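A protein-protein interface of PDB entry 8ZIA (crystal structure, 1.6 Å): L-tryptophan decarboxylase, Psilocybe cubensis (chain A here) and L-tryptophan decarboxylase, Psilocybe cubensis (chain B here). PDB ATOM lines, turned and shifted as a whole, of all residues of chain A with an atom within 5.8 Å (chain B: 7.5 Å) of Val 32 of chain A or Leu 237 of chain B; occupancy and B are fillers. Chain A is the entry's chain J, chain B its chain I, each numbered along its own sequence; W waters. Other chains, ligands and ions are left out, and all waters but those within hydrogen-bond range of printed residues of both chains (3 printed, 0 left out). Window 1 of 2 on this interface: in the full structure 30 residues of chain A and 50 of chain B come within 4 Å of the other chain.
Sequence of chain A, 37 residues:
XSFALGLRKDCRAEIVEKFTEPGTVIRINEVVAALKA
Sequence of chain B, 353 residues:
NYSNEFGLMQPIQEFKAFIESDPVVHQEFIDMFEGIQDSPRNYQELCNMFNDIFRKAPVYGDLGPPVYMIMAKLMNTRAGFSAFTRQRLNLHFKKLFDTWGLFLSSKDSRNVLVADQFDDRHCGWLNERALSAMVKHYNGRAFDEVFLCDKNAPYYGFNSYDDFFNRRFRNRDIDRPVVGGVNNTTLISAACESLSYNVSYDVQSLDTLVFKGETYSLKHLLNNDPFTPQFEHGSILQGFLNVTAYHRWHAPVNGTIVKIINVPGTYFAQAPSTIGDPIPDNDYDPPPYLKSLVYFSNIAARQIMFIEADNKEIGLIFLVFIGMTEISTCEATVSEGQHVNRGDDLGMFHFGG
The backbone NH (N) of Ser 189 of chain B lies within hydrogen-bond range of the backbone carbonyl oxygen (O) of Pro 252 of chain B, at 2.7 Å.
Of the 26 printed residues of chain B, 18 touch a printed residue of chain A. Along chain B the printed residues that touch a printed residue of chain A span positions 187 to 342. Among the printed residues, 40 pairs touch across the chains. Among the printed residues, no Asp or Glu carboxylate lies within 4 Å of a Lys or Arg side-chain nitrogen of the other chain.
Of chain B, only Ile 188, Ser 189, Ala 190 and Leu 237 come within 4 Å of Val 32 of chain A. Printed residues of chain B within 4 Å of Ala 34 of chain A: Leu 187 (3.7 Å). Leu 237 of chain B touches just these residues of chain A: Phe 3, Ala 4, Leu 5, Ile 15 and Val 32. Pro 252 of chain B touches none of the printed residues of chain A. Printed residues of chain A within 4 Å of Arg 342 of chain B: Val 31 (3.96 Å). The nearest residue of chain B that does not touch Val 32 of chain A is Ala 191 of chain B (5.8 Å). The nearest printed residue of chain A that does not touch Val 320 of chain B is Leu 5 of chain A (5.1 Å).
Water W3 lies within hydrogen-bond range of the backbone carbonyl oxygen (O) of Ser 194 of chain B and the backbone carbonyl oxygen (O) of Ile 26 of chain A.
O of Ile 188 of chain B sits at hydrogen-bond distance from N of Val 32 of chain A (2.8 Å). O of Ala 33 of chain A sits at hydrogen-bond distance from N of Ile 188 of chain B (2.9 Å). N of Ala 190 of chain B lies within hydrogen-bond range of O of Glu 30 of chain A (2.9 Å). The backbone carbonyl oxygen of Ser 194 of chain B is in hydrogen-bond range of the backbone NH of Ile 26 of chain A (2.8 Å). N of Leu 5 of chain A is in hydrogen-bond range of O of Leu 237 of chain B, at 2.7 Å. O of Phe 3 of chain A sits at hydrogen-bond distance from N of Gly 239 of chain B. O of Phe 318 of chain B lies within hydrogen-bond range of N of Gly 6 of chain A, at 2.8 Å. N of Ala 4 of chain A lies within hydrogen-bond range of O of Val 320 of chain B, at 2.9 Å.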
ATOM      1  N   PHE A   3     -28.039  -7.452  16.457  1.00  0.00           N
ATOM      2  CA  PHE A   3     -27.843  -6.013  16.440  1.00  0.00           C
ATOM      3  C   PHE A   3     -28.306  -5.489  15.100  1.00  0.00           C
ATOM      4  O   PHE A   3     -28.305  -6.217  14.101  1.00  0.00           O
ATOM      5  CB  PHE A   3     -26.375  -5.620  16.681  1.00  0.00           C
ATOM      6  CG  PHE A   3     -25.520  -5.655  15.450  1.00  0.00           C
ATOM      7  CD1 PHE A   3     -25.043  -6.858  14.947  1.00  0.00           C
ATOM      8  CD2 PHE A   3     -25.182  -4.478  14.795  1.00  0.00           C
ATOM      9  CE1 PHE A   3     -24.245  -6.892  13.806  1.00  0.00           C
ATOM     10  CE2 PHE A   3     -24.387  -4.500  13.658  1.00  0.00           C
ATOM     11  CZ  PHE A   3     -23.918  -5.712  13.158  1.00  0.00           C
ATOM     12  N   ALA A   4     -28.710  -4.230  15.103  1.00  0.00           N
ATOM     13  CA  ALA A   4     -29.130  -3.549  13.893  1.00  0.00           C
ATOM     14  C   ALA A   4     -28.364  -2.250  13.789  1.00  0.00           C
ATOM     15  O   ALA A   4     -28.210  -1.534  14.778  1.00  0.00           O
ATOM     16  CB  ALA A   4     -30.630  -3.273  13.893  1.00  0.00           C
ATOM     17  N   LEU A   5     -27.910  -1.954  12.576  1.00  0.00           N
ATOM     18  CA  LEU A   5     -27.288  -0.686  12.224  1.00  0.00           C
ATOM     19  C   LEU A   5     -28.270   0.070  11.352  1.00  0.00           C
ATOM     20  O   LEU A   5     -28.736  -0.467  10.347  1.00  0.00           O
ATOM     21  CB  LEU A   5     -25.975  -0.919  11.470  1.00  0.00           C
ATOM     22  CG  LEU A   5     -25.357   0.279  10.743  1.00  0.00           C
ATOM     23  CD1 LEU A   5     -24.814   1.291  11.749  1.00  0.00           C
ATOM     24  CD2 LEU A   5     -24.270  -0.148   9.738  1.00  0.00           C
ATOM     25  N   GLY A   6     -28.584   1.298  11.746  1.00  0.00           N
ATOM     26  CA  GLY A   6     -29.535   2.116  11.007  1.00  0.00           C
ATOM     27  C   GLY A   6     -28.870   3.332  10.396  1.00  0.00           C
ATOM     28  O   GLY A   6     -28.168   4.081  11.086  1.00  0.00           O
ATOM     29  N   GLU A  14     -23.349   3.471   2.025  1.00  0.00           N
ATOM     30  CA  GLU A  14     -24.352   2.483   1.669  1.00  0.00           C
ATOM     31  C   GLU A  14     -23.893   1.108   2.128  1.00  0.00           C
ATOM     32  O   GLU A  14     -22.700   0.792   2.071  1.00  0.00           O
ATOM     33  CB  GLU A  14     -24.598   2.458   0.162  1.00  0.00           C
ATOM     34  CG  GLU A  14     -25.241   3.710  -0.384  1.00  0.00           C
ATOM     35  CD  GLU A  14     -25.356   3.675  -1.897  1.00  0.00           C
ATOM     36  OE1 GLU A  14     -24.791   2.744  -2.514  1.00  0.00           O
ATOM     37  OE2 GLU A  14     -26.011   4.571  -2.467  1.00  0.00           O
ATOM     38  N   ILE A  15     -24.857   0.291   2.555  1.00  0.00           N
ATOM     39  CA  ILE A  15     -24.552  -1.050   3.041  1.00  0.00           C
ATOM     40  C   ILE A  15     -23.853  -1.866   1.959  1.00  0.00           C
ATOM     41  O   ILE A  15     -24.240  -1.852   0.780  1.00  0.00           O
ATOM     42  CB  ILE A  15     -25.845  -1.724   3.530  1.00  0.00           C
ATOM     43  CG1 ILE A  15     -26.385  -0.965   4.742  1.00  0.00           C
ATOM     44  CG2 ILE A  15     -25.594  -3.184   3.901  1.00  0.00           C
ATOM     45  CD1 ILE A  15     -27.832  -1.271   5.064  1.00  0.00           C
ATOM     46  N   VAL A  16     -22.802  -2.580   2.365  1.00  0.00           N
ATOM     47  CA  VAL A  16     -22.020  -3.386   1.433  1.00  0.00           C
ATOM     48  C   VAL A  16     -22.874  -4.536   0.917  1.00  0.00           C
ATOM     49  O   VAL A  16     -23.514  -5.260   1.692  1.00  0.00           O
ATOM     50  CB  VAL A  16     -20.736  -3.888   2.110  1.00  0.00           C
ATOM     51  CG1 VAL A  16     -20.038  -4.925   1.235  1.00  0.00           C
ATOM     52  CG2 VAL A  16     -19.805  -2.711   2.387  1.00  0.00           C
ATOM     53  N   PHE A  19     -23.699  -8.288   2.183  1.00  0.00           N
ATOM     54  CA  PHE A  19     -24.426  -8.547   3.418  1.00  0.00           C
ATOM     55  C   PHE A  19     -25.934  -8.589   3.231  1.00  0.00           C
ATOM     56  O   PHE A  19     -26.643  -8.944   4.182  1.00  0.00           O
ATOM     57  CB  PHE A  19     -24.029  -7.510   4.469  1.00  0.00           C
ATOM     58  CG  PHE A  19     -22.563  -7.547   4.791  1.00  0.00           C
ATOM     59  CD1 PHE A  19     -21.994  -8.688   5.329  1.00  0.00           C
ATOM     60  CD2 PHE A  19     -21.753  -6.458   4.523  1.00  0.00           C
ATOM     61  CE1 PHE A  19     -20.647  -8.739   5.607  1.00  0.00           C
ATOM     62  CE2 PHE A  19     -20.398  -6.499   4.797  1.00  0.00           C
ATOM     63  CZ  PHE A  19     -19.847  -7.639   5.348  1.00  0.00           C
ATOM     64  N   ILE A  26     -20.179 -11.925   8.990  1.00  0.00           N
ATOM     65  CA  ILE A  26     -19.824 -10.555   9.346  1.00  0.00           C
ATOM     66  C   ILE A  26     -18.692 -10.637  10.363  1.00  0.00           C
ATOM     67  O   ILE A  26     -18.910 -10.951  11.541  1.00  0.00           O
ATOM     68  CB  ILE A  26     -21.013  -9.778   9.919  1.00  0.00           C
ATOM     69  CG1 ILE A  26     -22.128  -9.670   8.889  1.00  0.00           C
ATOM     70  CG2 ILE A  26     -20.550  -8.376  10.351  1.00  0.00           C
ATOM     71  CD1 ILE A  26     -23.414  -9.077   9.459  1.00  0.00           C
ATOM     72  N   GLU A  30     -15.005  -5.401  10.253  1.00  0.00           N
ATOM     73  CA  GLU A  30     -14.903  -5.251   8.808  1.00  0.00           C
ATOM     74  C   GLU A  30     -15.919  -4.224   8.323  1.00  0.00           C
ATOM     75  O   GLU A  30     -16.873  -3.881   9.021  1.00  0.00           O
ATOM     76  CB  GLU A  30     -15.082  -6.595   8.091  1.00  0.00           C
ATOM     77  CG  GLU A  30     -16.519  -7.077   7.861  1.00  0.00           C
ATOM     78  CD  GLU A  30     -16.547  -8.283   6.919  1.00  0.00           C
ATOM     79  OE1 GLU A  30     -16.211  -8.124   5.720  1.00  0.00           O
ATOM     80  OE2 GLU A  30     -16.881  -9.398   7.369  1.00  0.00           O
ATOM     81  N   VAL A  31     -15.698  -3.718   7.111  1.00  0.00           N
ATOM     82  CA  VAL A  31     -16.552  -2.659   6.588  1.00  0.00           C
ATOM     83  C   VAL A  31     -17.907  -3.231   6.215  1.00  0.00           C
ATOM     84  O   VAL A  31     -18.002  -4.211   5.462  1.00  0.00           O
ATOM     85  CB  VAL A  31     -15.886  -1.994   5.376  1.00  0.00           C
ATOM     86  CG1 VAL A  31     -16.830  -0.974   4.741  1.00  0.00           C
ATOM     87  CG2 VAL A  31     -14.586  -1.334   5.803  1.00  0.00           C
ATOM     88  N   VAL A  32     -18.972  -2.613   6.726  1.00  0.00           N
ATOM     89  CA  VAL A  32     -20.325  -2.988   6.330  1.00  0.00           C
ATOM     90  C   VAL A  32     -21.048  -1.881   5.583  1.00  0.00           C
ATOM     91  O   VAL A  32     -22.097  -2.153   4.984  1.00  0.00           O
ATOM     92  CB  VAL A  32     -21.166  -3.452   7.539  1.00  0.00           C
ATOM     93  CG1 VAL A  32     -20.547  -4.715   8.140  1.00  0.00           C
ATOM     94  CG2 VAL A  32     -21.278  -2.342   8.571  1.00  0.00           C
ATOM     95  N   ALA A  33     -20.532  -0.651   5.593  1.00  0.00           N
ATOM     96  CA  ALA A  33     -21.114   0.423   4.798  1.00  0.00           C
ATOM     97  C   ALA A  33     -20.010   1.408   4.448  1.00  0.00           C
ATOM     98  O   ALA A  33     -19.078   1.616   5.231  1.00  0.00           O
ATOM     99  CB  ALA A  33     -22.257   1.121   5.546  1.00  0.00           C
ATOM    100  N   ALA A  34     -20.118   2.009   3.263  1.00  0.00           N
ATOM    101  CA  ALA A  34     -19.045   2.853   2.760  1.00  0.00           C
ATOM    102  C   ALA A  34     -19.629   3.817   1.742  1.00  0.00           C
ATOM    103  O   ALA A  34     -20.689   3.557   1.168  1.00  0.00           O
ATOM    104  CB  ALA A  34     -17.930   2.017   2.131  1.00  0.00           C
ATOM    105  N   LEU B 187     -15.888   5.222   6.501  1.00  0.00           N
ATOM    106  CA  LEU B 187     -16.167   3.794   6.560  1.00  0.00           C
ATOM    107  C   LEU B 187     -16.935   3.474   7.833  1.00  0.00           C
ATOM    108  O   LEU B 187     -16.700   4.081   8.885  1.00  0.00           O
ATOM    109  CB  LEU B 187     -14.869   2.982   6.518  1.00  0.00           C
ATOM    110  CG  LEU B 187     -14.032   3.148   5.243  1.00  0.00           C
ATOM    111  CD1 LEU B 187     -12.715   2.391   5.362  1.00  0.00           C
ATOM    112  CD2 LEU B 187     -14.792   2.669   4.017  1.00  0.00           C
ATOM    113  N   ILE B 188     -17.862   2.529   7.723  1.00  0.00           N
ATOM    114  CA  ILE B 188     -18.632   2.034   8.856  1.00  0.00           C
ATOM    115  C   ILE B 188     -18.348   0.551   9.008  1.00  0.00           C
ATOM    116  O   ILE B 188     -18.494  -0.213   8.041  1.00  0.00           O
ATOM    117  CB  ILE B 188     -20.137   2.273   8.665  1.00  0.00           C
ATOM    118  CG1 ILE B 188     -20.397   3.757   8.393  1.00  0.00           C
ATOM    119  CG2 ILE B 188     -20.902   1.756   9.898  1.00  0.00           C
ATOM    120  CD1 ILE B 188     -21.901   4.111   8.289  1.00  0.00           C
ATOM    121  N   SER B 189     -17.953   0.146  10.219  1.00  0.00           N
ATOM    122  CA  SER B 189     -17.590  -1.227  10.529  1.00  0.00           C
ATOM    123  C   SER B 189     -18.729  -1.957  11.229  1.00  0.00           C
ATOM    124  O   SER B 189     -19.617  -1.344  11.833  1.00  0.00           O
ATOM    125  CB  SER B 189     -16.352  -1.282  11.433  1.00  0.00           C
ATOM    126  OG  SER B 189     -15.164  -1.139  10.698  1.00  0.00           O
ATOM    127  N   ALA B 190     -18.669  -3.286  11.153  1.00  0.00           N
ATOM    128  CA  ALA B 190     -19.577  -4.138  11.910  1.00  0.00           C
ATOM    129  C   ALA B 190     -19.339  -3.989  13.407  1.00  0.00           C
ATOM    130  O   ALA B 190     -18.214  -4.143  13.883  1.00  0.00           O
ATOM    131  CB  ALA B 190     -19.396  -5.599  11.505  1.00  0.00           C
ATOM    132  N   ALA B 191     -20.406  -3.715  14.152  1.00  0.00           N
ATOM    133  CA  ALA B 191     -20.305  -3.543  15.593  1.00  0.00           C
ATOM    134  C   ALA B 191     -20.236  -4.866  16.333  1.00  0.00           C
ATOM    135  O   ALA B 191     -19.794  -4.889  17.494  1.00  0.00           O
ATOM    136  CB  ALA B 191     -21.497  -2.728  16.120  1.00  0.00           C
ATOM    137  N   CYS B 192     -20.664  -5.957  15.697  1.00  0.00           N
ATOM    138  CA  CYS B 192     -20.703  -7.272  16.318  1.00  0.00           C
ATOM    139  C   CYS B 192     -20.228  -8.329  15.343  1.00  0.00           C
ATOM    140  O   CYS B 192     -20.464  -8.228  14.135  1.00  0.00           O
ATOM    141  CB  CYS B 192     -22.112  -7.671  16.764  1.00  0.00           C
ATOM    142  SG  CYS B 192     -22.770  -6.670  18.095  1.00  0.00           S
ATOM    143  N   SER B 194     -20.825 -11.640  13.736  1.00  0.00           N
ATOM    144  CA  SER B 194     -22.199 -12.073  13.506  1.00  0.00           C
ATOM    145  C   SER B 194     -22.328 -12.738  12.142  1.00  0.00           C
ATOM    146  O   SER B 194     -21.365 -12.851  11.378  1.00  0.00           O
ATOM    147  CB  SER B 194     -23.159 -10.878  13.631  1.00  0.00           C
ATOM    148  OG  SER B 194     -22.695  -9.771  12.865  1.00  0.00           O
ATOM    149  N   LEU B 195     -23.547 -13.175  11.843  1.00  0.00           N
ATOM    150  CA  LEU B 195     -23.951 -13.578  10.504  1.00  0.00           C
ATOM    151  C   LEU B 195     -25.017 -12.602  10.029  1.00  0.00           C
ATOM    152  O   LEU B 195     -25.885 -12.193  10.806  1.00  0.00           O
ATOM    153  CB  LEU B 195     -24.512 -15.006  10.494  1.00  0.00           C
ATOM    154  CG  LEU B 195     -23.535 -16.086  10.955  1.00  0.00           C
ATOM    155  CD1 LEU B 195     -24.245 -17.418  11.149  1.00  0.00           C
ATOM    156  CD2 LEU B 195     -22.421 -16.209   9.933  1.00  0.00           C
ATOM    157  N   SER B 196     -24.939 -12.188   8.768  1.00  0.00           N
ATOM    158  CA  SER B 196     -25.974 -11.297   8.280  1.00  0.00           C
ATOM    159  C   SER B 196     -27.331 -11.971   8.409  1.00  0.00           C
ATOM    160  O   SER B 196     -27.478 -13.172   8.157  1.00  0.00           O
ATOM    161  CB  SER B 196     -25.705 -10.905   6.831  1.00  0.00           C
ATOM    162  OG  SER B 196     -25.842 -12.040   6.001  1.00  0.00           O
ATOM    163  N   TYR B 197     -28.318 -11.206   8.862  1.00  0.00           N
ATOM    164  CA  TYR B 197     -29.677 -11.715   8.965  1.00  0.00           C
ATOM    165  C   TYR B 197     -30.623 -11.046   7.989  1.00  0.00           C
ATOM    166  O   TYR B 197     -31.404 -11.728   7.322  1.00  0.00           O
ATOM    167  CB  TYR B 197     -30.213 -11.530  10.391  1.00  0.00           C
ATOM    168  CG  TYR B 197     -31.527 -12.234  10.580  1.00  0.00           C
ATOM    169  CD1 TYR B 197     -31.565 -13.577  10.943  1.00  0.00           C
ATOM    170  CD2 TYR B 197     -32.725 -11.567  10.366  1.00  0.00           C
ATOM    171  CE1 TYR B 197     -32.764 -14.230  11.100  1.00  0.00           C
ATOM    172  CE2 TYR B 197     -33.937 -12.216  10.517  1.00  0.00           C
ATOM    173  CZ  TYR B 197     -33.942 -13.542  10.887  1.00  0.00           C
ATOM    174  OH  TYR B 197     -35.157 -14.174  11.035  1.00  0.00           O
ATOM    175  N   ASN B 198     -30.553  -9.726   7.881  1.00  0.00           N
ATOM    176  CA  ASN B 198     -31.474  -9.011   7.018  1.00  0.00           C
ATOM    177  C   ASN B 198     -30.913  -7.647   6.674  1.00  0.00           C
ATOM    178  O   ASN B 198     -30.278  -6.993   7.503  1.00  0.00           O
ATOM    179  CB  ASN B 198     -32.831  -8.853   7.699  1.00  0.00           C
ATOM    180  CG  ASN B 198     -33.799  -8.078   6.852  1.00  0.00           C
ATOM    181  OD1 ASN B 198     -34.251  -8.570   5.822  1.00  0.00           O
ATOM    182  ND2 ASN B 198     -34.098  -6.853   7.258  1.00  0.00           N
ATOM    183  N   VAL B 199     -31.185  -7.202   5.447  1.00  0.00           N
ATOM    184  CA  VAL B 199     -30.992  -5.812   5.066  1.00  0.00           C
ATOM    185  C   VAL B 199     -32.318  -5.315   4.511  1.00  0.00           C
ATOM    186  O   VAL B 199     -32.911  -5.973   3.649  1.00  0.00           O
ATOM    187  CB  VAL B 199     -29.869  -5.620   4.024  1.00  0.00           C
ATOM    188  CG1 VAL B 199     -29.871  -4.169   3.535  1.00  0.00           C
ATOM    189  CG2 VAL B 199     -28.496  -6.002   4.622  1.00  0.00           C
ATOM    190  N   SER B 200     -32.798  -4.189   5.033  1.00  0.00           N
ATOM    191  CA  SER B 200     -34.012  -3.553   4.536  1.00  0.00           C
ATOM    192  C   SER B 200     -33.718  -2.133   4.089  1.00  0.00           C
ATOM    193  O   SER B 200     -32.964  -1.403   4.740  1.00  0.00           O
ATOM    194  CB  SER B 200     -35.123  -3.518   5.601  1.00  0.00           C
ATOM    195  OG  SER B 200     -35.674  -4.801   5.806  1.00  0.00           O
ATOM    196  N   VAL B 203     -36.949   2.110   5.009  1.00  0.00           N
ATOM    197  CA  VAL B 203     -37.663   1.625   6.183  1.00  0.00           C
ATOM    198  C   VAL B 203     -38.640   2.683   6.697  1.00  0.00           C
ATOM    199  O   VAL B 203     -38.499   3.888   6.458  1.00  0.00           O
ATOM    200  CB  VAL B 203     -36.660   1.204   7.267  1.00  0.00           C
ATOM    201  CG1 VAL B 203     -35.744   0.087   6.747  1.00  0.00           C
ATOM    202  CG2 VAL B 203     -35.868   2.411   7.740  1.00  0.00           C
ATOM    203  N   TYR B 216     -39.459  -4.198   9.967  1.00  0.00           N
ATOM    204  CA  TYR B 216     -39.151  -3.163  10.949  1.00  0.00           C
ATOM    205  C   TYR B 216     -40.254  -2.122  11.014  1.00  0.00           C
ATOM    206  O   TYR B 216     -40.826  -1.736   9.987  1.00  0.00           O
ATOM    207  CB  TYR B 216     -37.859  -2.428  10.621  1.00  0.00           C
ATOM    208  CG  TYR B 216     -36.662  -3.330  10.483  1.00  0.00           C
ATOM    209  CD1 TYR B 216     -36.043  -3.507   9.250  1.00  0.00           C
ATOM    210  CD2 TYR B 216     -36.163  -4.023  11.577  1.00  0.00           C
ATOM    211  CE1 TYR B 216     -34.961  -4.319   9.104  1.00  0.00           C
ATOM    212  CE2 TYR B 216     -35.055  -4.837  11.443  1.00  0.00           C
ATOM    213  CZ  TYR B 216     -34.480  -4.995  10.198  1.00  0.00           C
ATOM    214  OH  TYR B 216     -33.393  -5.818  10.064  1.00  0.00           O
ATOM    215  N   SER B 235     -32.064   2.880   5.842  1.00  0.00           N
ATOM    216  CA  SER B 235     -31.765   1.473   5.638  1.00  0.00           C
ATOM    217  C   SER B 235     -31.262   0.866   6.939  1.00  0.00           C
ATOM    218  O   SER B 235     -30.728   1.566   7.801  1.00  0.00           O
ATOM    219  CB  SER B 235     -30.728   1.256   4.523  1.00  0.00           C
ATOM    220  OG  SER B 235     -29.541   1.992   4.769  1.00  0.00           O
ATOM    221  N   ILE B 236     -31.455  -0.436   7.075  1.00  0.00           N
ATOM    222  CA  ILE B 236     -31.041  -1.164   8.270  1.00  0.00           C
ATOM    223  C   ILE B 236     -30.326  -2.447   7.867  1.00  0.00           C
ATOM    224  O   ILE B 236     -30.811  -3.197   7.011  1.00  0.00           O
ATOM    225  CB  ILE B 236     -32.241  -1.487   9.177  1.00  0.00           C
ATOM    226  CG1 ILE B 236     -32.818  -0.199   9.752  1.00  0.00           C
ATOM    227  CG2 ILE B 236     -31.811  -2.471  10.298  1.00  0.00           C
ATOM    228  CD1 ILE B 236     -34.119  -0.430  10.507  1.00  0.00           C
ATOM    229  N   LEU B 237     -29.183  -2.707   8.503  1.00  0.00           N
ATOM    230  CA  LEU B 237     -28.493  -3.985   8.444  1.00  0.00           C
ATOM    231  C   LEU B 237     -28.605  -4.652   9.809  1.00  0.00           C
ATOM    232  O   LEU B 237     -28.302  -4.029  10.830  1.00  0.00           O
ATOM    233  CB  LEU B 237     -27.011  -3.797   8.082  1.00  0.00           C
ATOM    234  CG  LEU B 237     -26.041  -4.953   8.381  1.00  0.00           C
ATOM    235  CD1 LEU B 237     -26.338  -6.178   7.498  1.00  0.00           C
ATOM    236  CD2 LEU B 237     -24.594  -4.484   8.193  1.00  0.00           C
ATOM    237  N   GLN B 238     -29.047  -5.901   9.830  1.00  0.00           N
ATOM    238  CA  GLN B 238     -29.203  -6.641  11.077  1.00  0.00           C
ATOM    239  C   GLN B 238     -28.392  -7.924  11.007  1.00  0.00           C
ATOM    240  O   GLN B 238     -28.444  -8.636   9.998  1.00  0.00           O
ATOM    241  CB  GLN B 238     -30.678  -6.959  11.334  1.00  0.00           C
ATOM    242  CG  GLN B 238     -30.903  -7.669  12.654  1.00  0.00           C
ATOM    243  CD  GLN B 238     -32.365  -7.827  12.979  1.00  0.00           C
ATOM    244  OE1 GLN B 238     -33.233  -7.458  12.187  1.00  0.00           O
ATOM    245  NE2 GLN B 238     -32.652  -8.371  14.158  1.00  0.00           N
ATOM    246  N   GLY B 239     -27.654  -8.216  12.084  1.00  0.00           N
ATOM    247  CA  GLY B 239     -26.847  -9.421  12.198  1.00  0.00           C
ATOM    248  C   GLY B 239     -27.286 -10.284  13.365  1.00  0.00           C
ATOM    249  O   GLY B 239     -27.942  -9.801  14.302  1.00  0.00           O
ATOM    250  N   PRO B 252     -18.875   1.402  15.521  1.00  0.00           N
ATOM    251  CA  PRO B 252     -18.939   1.186  14.069  1.00  0.00           C
ATOM    252  C   PRO B 252     -18.360   2.327  13.262  1.00  0.00           C
ATOM    253  O   PRO B 252     -18.115   2.147  12.061  1.00  0.00           O
ATOM    254  CB  PRO B 252     -20.446   1.061  13.807  1.00  0.00           C
ATOM    255  CG  PRO B 252     -21.038   1.956  14.866  1.00  0.00           C
ATOM    256  CD  PRO B 252     -20.204   1.682  16.095  1.00  0.00           C
ATOM    257  N   PHE B 318     -27.834   4.927  14.016  1.00  0.00           N
ATOM    258  CA  PHE B 318     -28.202   4.223  15.236  1.00  0.00           C
ATOM    259  C   PHE B 318     -27.698   2.789  15.220  1.00  0.00           C
ATOM    260  O   PHE B 318     -27.474   2.173  14.170  1.00  0.00           O
ATOM    261  CB  PHE B 318     -29.739   4.265  15.537  1.00  0.00           C
ATOM    262  CG  PHE B 318     -30.624   3.442  14.615  1.00  0.00           C
ATOM    263  CD1 PHE B 318     -30.650   2.052  14.675  1.00  0.00           C
ATOM    264  CD2 PHE B 318     -31.543   4.090  13.778  1.00  0.00           C
ATOM    265  CE1 PHE B 318     -31.508   1.308  13.861  1.00  0.00           C
ATOM    266  CE2 PHE B 318     -32.412   3.360  12.967  1.00  0.00           C
ATOM    267  CZ  PHE B 318     -32.407   1.976  13.004  1.00  0.00           C
ATOM    268  N   LEU B 319     -27.472   2.287  16.423  1.00  0.00           N
ATOM    269  CA  LEU B 319     -27.329   0.868  16.679  1.00  0.00           C
ATOM    270  C   LEU B 319     -28.443   0.457  17.618  1.00  0.00           C
ATOM    271  O   LEU B 319     -28.792   1.203  18.536  1.00  0.00           O
ATOM    272  CB  LEU B 319     -25.978   0.541  17.332  1.00  0.00           C
ATOM    273  CG  LEU B 319     -24.749   0.834  16.493  1.00  0.00           C
ATOM    274  CD1 LEU B 319     -23.544   0.898  17.416  1.00  0.00           C
ATOM    275  CD2 LEU B 319     -24.577  -0.269  15.454  1.00  0.00           C
ATOM    276  N   VAL B 320     -29.006  -0.722  17.397  1.00  0.00           N
ATOM    277  CA  VAL B 320     -29.859  -1.346  18.399  1.00  0.00           C
ATOM    278  C   VAL B 320     -29.256  -2.695  18.737  1.00  0.00           C
ATOM    279  O   VAL B 320     -29.033  -3.528  17.849  1.00  0.00           O
ATOM    280  CB  VAL B 320     -31.311  -1.491  17.930  1.00  0.00           C
ATOM    281  CG1 VAL B 320     -32.182  -2.041  19.077  1.00  0.00           C
ATOM    282  CG2 VAL B 320     -31.815  -0.147  17.439  1.00  0.00           C
ATOM    283  N   ILE B 322     -30.015  -6.052  20.472  1.00  0.00           N
ATOM    284  CA  ILE B 322     -31.317  -6.706  20.566  1.00  0.00           C
ATOM    285  C   ILE B 322     -31.142  -7.979  21.384  1.00  0.00           C
ATOM    286  O   ILE B 322     -30.373  -8.871  21.000  1.00  0.00           O
ATOM    287  CB  ILE B 322     -31.872  -7.020  19.169  1.00  0.00           C
ATOM    288  CG1 ILE B 322     -32.028  -5.731  18.340  1.00  0.00           C
ATOM    289  CG2 ILE B 322     -33.219  -7.771  19.282  1.00  0.00           C
ATOM    290  CD1 ILE B 322     -31.967  -5.974  16.840  1.00  0.00           C
ATOM    291  N   ARG B 342     -13.719   4.025  15.355  1.00  0.00           N
ATOM    292  CA  ARG B 342     -14.137   2.751  14.791  1.00  0.00           C
ATOM    293  C   ARG B 342     -13.252   1.620  15.321  1.00  0.00           C
ATOM    294  O   ARG B 342     -12.021   1.695  15.266  1.00  0.00           O
ATOM    295  CB  ARG B 342     -14.071   2.846  13.260  1.00  0.00           C
ATOM    296  CG  ARG B 342     -14.691   1.689  12.517  1.00  0.00           C
ATOM    297  CD  ARG B 342     -14.899   2.040  11.049  1.00  0.00           C
ATOM    298  NE  ARG B 342     -13.636   2.350  10.383  1.00  0.00           N
ATOM    299  CZ  ARG B 342     -13.032   1.563   9.504  1.00  0.00           C
ATOM    300  NH1 ARG B 342     -13.501   0.356   9.217  1.00  0.00           N
ATOM    301  NH2 ARG B 342     -11.933   1.998   8.891  1.00  0.00           N
HETATM  302  O   HOH W   1     -27.596   1.468   2.691  1.00  0.00           O
HETATM  303  O   HOH W   2     -28.894 -10.425   5.090  1.00  0.00           O
HETATM  304  O   HOH W   3     -19.087 -14.333  12.289  1.00  0.00           O
